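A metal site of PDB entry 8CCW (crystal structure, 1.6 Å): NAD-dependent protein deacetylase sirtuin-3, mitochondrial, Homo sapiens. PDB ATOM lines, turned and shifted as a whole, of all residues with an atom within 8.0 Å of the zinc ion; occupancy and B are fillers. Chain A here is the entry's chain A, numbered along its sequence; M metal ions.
The backbone NH (N) of Cys 163 is in hydrogen-bond range of the backbone carbonyl oxygen (O) of Gly 168, at 2.8 Å. The side-chain sulfur (SG) of Cys 163 lies close to the backbone NH (N) of Val 165, 3.4 Å away. N of Gly 168 lies close to SG of Cys 166, at 3.3 Å. SG of Cys 142 sits close to NH1 of Arg 144 (3.4 Å). The backbone NH (N) of Val 141 lies close to the side-chain sulfur (SG) of Cys 139 (3.4 Å). The backbone carbonyl oxygen of Arg 144 sits at hydrogen-bond distance from the backbone NH of Cys 139. The backbone carbonyl oxygen of Cys 139 is in hydrogen-bond range of the side-chain amide nitrogen of Gln 143, at 3.0 Å.
Within 4 Å of the zinc ion: Cys 139, Cys 142, Cys 163 and Cys 166.
The zinc ion is bound by SG of Cys 163 (2.3 Å), SG of Cys 166 (2.3 Å), SG of Cys 142 (2.3 Å) and SG of Cys 139 (2.4 Å).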
ATOM      1  N   THR A 138     -24.665 -19.395   2.563  1.00  0.00           N
ATOM      2  CA  THR A 138     -23.819 -18.905   3.638  1.00  0.00           C
ATOM      3  C   THR A 138     -24.013 -17.404   3.767  1.00  0.00           C
ATOM      4  O   THR A 138     -23.998 -16.708   2.753  1.00  0.00           O
ATOM      5  CB  THR A 138     -22.336 -19.181   3.349  1.00  0.00           C
ATOM      6  OG1 THR A 138     -22.145 -20.588   3.140  1.00  0.00           O
ATOM      7  CG2 THR A 138     -21.499 -18.721   4.513  1.00  0.00           C
ATOM      8  N   CYS A 139     -24.214 -16.910   4.992  1.00  0.00           N
ATOM      9  CA  CYS A 139     -24.259 -15.442   5.170  1.00  0.00           C
ATOM     10  C   CYS A 139     -22.927 -14.800   4.801  1.00  0.00           C
ATOM     11  O   CYS A 139     -21.847 -15.228   5.245  1.00  0.00           O
ATOM     12  CB  CYS A 139     -24.602 -15.078   6.614  1.00  0.00           C
ATOM     13  SG  CYS A 139     -24.632 -13.270   6.825  1.00  0.00           S
ATOM     14  N   THR A 140     -22.985 -13.793   3.921  1.00  0.00           N
ATOM     15  CA  THR A 140     -21.755 -13.150   3.474  1.00  0.00           C
ATOM     16  C   THR A 140     -21.059 -12.326   4.564  1.00  0.00           C
ATOM     17  O   THR A 140     -19.884 -11.963   4.396  1.00  0.00           O
ATOM     18  CB  THR A 140     -22.039 -12.232   2.281  1.00  0.00           C
ATOM     19  OG1 THR A 140     -23.043 -11.261   2.676  1.00  0.00           O
ATOM     20  CG2 THR A 140     -22.565 -13.073   1.079  1.00  0.00           C
ATOM     21  N   VAL A 141     -21.760 -12.007   5.644  1.00  0.00           N
ATOM     22  CA  VAL A 141     -21.175 -11.239   6.729  1.00  0.00           C
ATOM     23  C   VAL A 141     -20.741 -12.155   7.870  1.00  0.00           C
ATOM     24  O   VAL A 141     -19.575 -12.152   8.268  1.00  0.00           O
ATOM     25  CB  VAL A 141     -22.165 -10.166   7.225  1.00  0.00           C
ATOM     26  CG1 VAL A 141     -21.608  -9.441   8.477  1.00  0.00           C
ATOM     27  CG2 VAL A 141     -22.431  -9.173   6.087  1.00  0.00           C
ATOM     28  N   CYS A 142     -21.676 -12.937   8.429  1.00  0.00           N
ATOM     29  CA  CYS A 142     -21.354 -13.675   9.663  1.00  0.00           C
ATOM     30  C   CYS A 142     -20.969 -15.114   9.403  1.00  0.00           C
ATOM     31  O   CYS A 142     -20.610 -15.827  10.370  1.00  0.00           O
ATOM     32  CB  CYS A 142     -22.541 -13.655  10.661  1.00  0.00           C
ATOM     33  SG  CYS A 142     -23.953 -14.666  10.291  1.00  0.00           S
ATOM     34  N   GLN A 143     -21.071 -15.579   8.162  1.00  0.00           N
ATOM     35  CA  GLN A 143     -20.663 -16.909   7.722  1.00  0.00           C
ATOM     36  C   GLN A 143     -21.552 -18.051   8.264  1.00  0.00           C
ATOM     37  O   GLN A 143     -21.204 -19.255   8.106  1.00  0.00           O
ATOM     38  CB  GLN A 143     -19.166 -17.101   8.063  1.00  0.00           C
ATOM     39  CG  GLN A 143     -18.035 -16.426   7.099  1.00  0.00           C
ATOM     40  CD  GLN A 143     -18.321 -15.090   6.286  1.00  0.00           C
ATOM     41  OE1 GLN A 143     -17.926 -13.973   6.731  1.00  0.00           O
ATOM     42  NE2 GLN A 143     -18.883 -15.221   5.041  1.00  0.00           N
ATOM     43  N   ARG A 144     -22.727 -17.749   8.814  1.00  0.00           N
ATOM     44  CA  ARG A 144     -23.709 -18.771   9.159  1.00  0.00           C
ATOM     45  C   ARG A 144     -24.181 -19.579   7.964  1.00  0.00           C
ATOM     46  O   ARG A 144     -24.588 -18.995   6.936  1.00  0.00           O
ATOM     47  CB  ARG A 144     -24.938 -18.112   9.831  1.00  0.00           C
ATOM     48  CG  ARG A 144     -24.842 -18.122  11.342  1.00  0.00           C
ATOM     49  CD  ARG A 144     -26.079 -17.533  12.060  1.00  0.00           C
ATOM     50  NE  ARG A 144     -25.868 -17.514  13.529  1.00  0.00           N
ATOM     51  CZ  ARG A 144     -25.093 -16.617  14.152  1.00  0.00           C
ATOM     52  NH1 ARG A 144     -24.452 -15.688  13.450  1.00  0.00           N
ATOM     53  NH2 ARG A 144     -24.963 -16.663  15.481  1.00  0.00           N
ATOM     54  N   PRO A 145     -24.230 -20.906   8.059  1.00  0.00           N
ATOM     55  CA  PRO A 145     -24.762 -21.716   6.954  1.00  0.00           C
ATOM     56  C   PRO A 145     -26.245 -21.952   7.066  1.00  0.00           C
ATOM     57  O   PRO A 145     -26.833 -21.998   8.152  1.00  0.00           O
ATOM     58  CB  PRO A 145     -23.982 -23.046   7.113  1.00  0.00           C
ATOM     59  CG  PRO A 145     -23.761 -23.143   8.645  1.00  0.00           C
ATOM     60  CD  PRO A 145     -23.573 -21.712   9.117  1.00  0.00           C
ATOM     61  N   PHE A 146     -26.854 -22.147   5.912  1.00  0.00           N
ATOM     62  CA  PHE A 146     -28.273 -22.407   5.804  1.00  0.00           C
ATOM     63  C   PHE A 146     -28.524 -23.475   4.765  1.00  0.00           C
ATOM     64  O   PHE A 146     -27.825 -23.520   3.734  1.00  0.00           O
ATOM     65  CB  PHE A 146     -29.050 -21.137   5.421  1.00  0.00           C
ATOM     66  CG  PHE A 146     -28.788 -19.980   6.370  1.00  0.00           C
ATOM     67  CD1 PHE A 146     -29.590 -19.806   7.522  1.00  0.00           C
ATOM     68  CD2 PHE A 146     -27.759 -19.082   6.125  1.00  0.00           C
ATOM     69  CE1 PHE A 146     -29.342 -18.735   8.408  1.00  0.00           C
ATOM     70  CE2 PHE A 146     -27.507 -17.988   6.985  1.00  0.00           C
ATOM     71  CZ  PHE A 146     -28.297 -17.829   8.149  1.00  0.00           C
ATOM     72  N   ARG A 162     -31.846 -12.398   3.293  1.00  0.00           N
ATOM     73  CA  ARG A 162     -31.036 -11.784   4.317  1.00  0.00           C
ATOM     74  C   ARG A 162     -30.912 -12.701   5.531  1.00  0.00           C
ATOM     75  O   ARG A 162     -31.816 -13.506   5.832  1.00  0.00           O
ATOM     76  CB  ARG A 162     -31.681 -10.464   4.779  1.00  0.00           C
ATOM     77  CG  ARG A 162     -31.823  -9.485   3.586  1.00  0.00           C
ATOM     78  CD  ARG A 162     -30.492  -8.798   3.600  1.00  0.00           C
ATOM     79  NE  ARG A 162     -30.343  -7.873   2.564  1.00  0.00           N
ATOM     80  CZ  ARG A 162     -29.373  -6.976   2.502  1.00  0.00           C
ATOM     81  NH1 ARG A 162     -28.433  -6.806   3.463  1.00  0.00           N
ATOM     82  NH2 ARG A 162     -29.374  -6.263   1.415  1.00  0.00           N
ATOM     83  N   CYS A 163     -29.811 -12.537   6.224  1.00  0.00           N
ATOM     84  CA  CYS A 163     -29.467 -13.379   7.363  1.00  0.00           C
ATOM     85  C   CYS A 163     -30.372 -13.028   8.546  1.00  0.00           C
ATOM     86  O   CYS A 163     -30.514 -11.847   8.866  1.00  0.00           O
ATOM     87  CB  CYS A 163     -28.045 -13.108   7.745  1.00  0.00           C
ATOM     88  SG  CYS A 163     -27.456 -14.044   9.229  1.00  0.00           S
ATOM     89  N   PRO A 164     -31.005 -13.995   9.193  1.00  0.00           N
ATOM     90  CA  PRO A 164     -31.921 -13.636  10.304  1.00  0.00           C
ATOM     91  C   PRO A 164     -31.184 -13.215  11.541  1.00  0.00           C
ATOM     92  O   PRO A 164     -31.830 -12.672  12.455  1.00  0.00           O
ATOM     93  CB  PRO A 164     -32.738 -14.936  10.538  1.00  0.00           C
ATOM     94  CG  PRO A 164     -31.877 -16.040  10.024  1.00  0.00           C
ATOM     95  CD  PRO A 164     -31.083 -15.436   8.862  1.00  0.00           C
ATOM     96  N   VAL A 165     -29.862 -13.402  11.616  1.00  0.00           N
ATOM     97  CA  VAL A 165     -29.114 -12.948  12.783  1.00  0.00           C
ATOM     98  C   VAL A 165     -28.462 -11.582  12.558  1.00  0.00           C
ATOM     99  O   VAL A 165     -28.547 -10.700  13.423  1.00  0.00           O
ATOM    100  CB  VAL A 165     -28.056 -13.987  13.217  1.00  0.00           C
ATOM    101  CG1 VAL A 165     -27.276 -13.419  14.398  1.00  0.00           C
ATOM    102  CG2 VAL A 165     -28.761 -15.329  13.619  1.00  0.00           C
ATOM    103  N   CYS A 166     -27.791 -11.354  11.415  1.00  0.00           N
ATOM    104  CA  CYS A 166     -27.054 -10.094  11.241  1.00  0.00           C
ATOM    105  C   CYS A 166     -27.539  -9.198  10.090  1.00  0.00           C
ATOM    106  O   CYS A 166     -27.053  -8.059   9.953  1.00  0.00           O
ATOM    107  CB  CYS A 166     -25.555 -10.337  11.046  1.00  0.00           C
ATOM    108  SG  CYS A 166     -25.128 -10.996   9.361  1.00  0.00           S
ATOM    109  N   THR A 167     -28.516  -9.661   9.305  1.00  0.00           N
ATOM    110  CA  THR A 167     -29.124  -9.039   8.122  1.00  0.00           C
ATOM    111  C   THR A 167     -28.183  -9.009   6.910  1.00  0.00           C
ATOM    112  O   THR A 167     -28.564  -8.444   5.893  1.00  0.00           O
ATOM    113  CB  THR A 167     -29.677  -7.603   8.313  1.00  0.00           C
ATOM    114  OG1 THR A 167     -28.597  -6.646   8.410  1.00  0.00           O
ATOM    115  CG2 THR A 167     -30.581  -7.527   9.540  1.00  0.00           C
ATOM    116  N   GLY A 168     -27.004  -9.635   6.968  1.00  0.00           N
ATOM    117  CA  GLY A 168     -26.174  -9.717   5.762  1.00  0.00           C
ATOM    118  C   GLY A 168     -26.896 -10.433   4.623  1.00  0.00           C
ATOM    119  O   GLY A 168     -27.787 -11.243   4.822  1.00  0.00           O
ATOM    120  N   VAL A 169     -26.460 -10.170   3.371  1.00  0.00           N
ATOM    121  CA  VAL A 169     -26.964 -10.953   2.247  1.00  0.00           C
ATOM    122  C   VAL A 169     -26.557 -12.410   2.420  1.00  0.00           C
ATOM    123  O   VAL A 169     -25.392 -12.700   2.711  1.00  0.00           O
ATOM    124  CB  VAL A 169     -26.451 -10.385   0.914  1.00  0.00           C
ATOM    125  CG1 VAL A 169     -26.891 -11.300  -0.254  1.00  0.00           C
ATOM    126  CG2 VAL A 169     -27.011  -8.957   0.675  1.00  0.00           C
ATOM    127  N   VAL A 170     -27.516 -13.329   2.237  1.00  0.00           N
ATOM    128  CA  VAL A 170     -27.203 -14.765   2.264  1.00  0.00           C
ATOM    129  C   VAL A 170     -26.967 -15.228   0.823  1.00  0.00           C
ATOM    130  O   VAL A 170     -27.867 -15.126  -0.023  1.00  0.00           O
ATOM    131  CB  VAL A 170     -28.323 -15.576   2.914  1.00  0.00           C
ATOM    132  CG1 VAL A 170     -27.977 -17.084   2.859  1.00  0.00           C
ATOM    133  CG2 VAL A 170     -28.424 -15.210   4.439  1.00  0.00           C
HETATM  134 ZN    ZN M   1     -25.331 -13.263   9.108  1.00  0.00          ZN
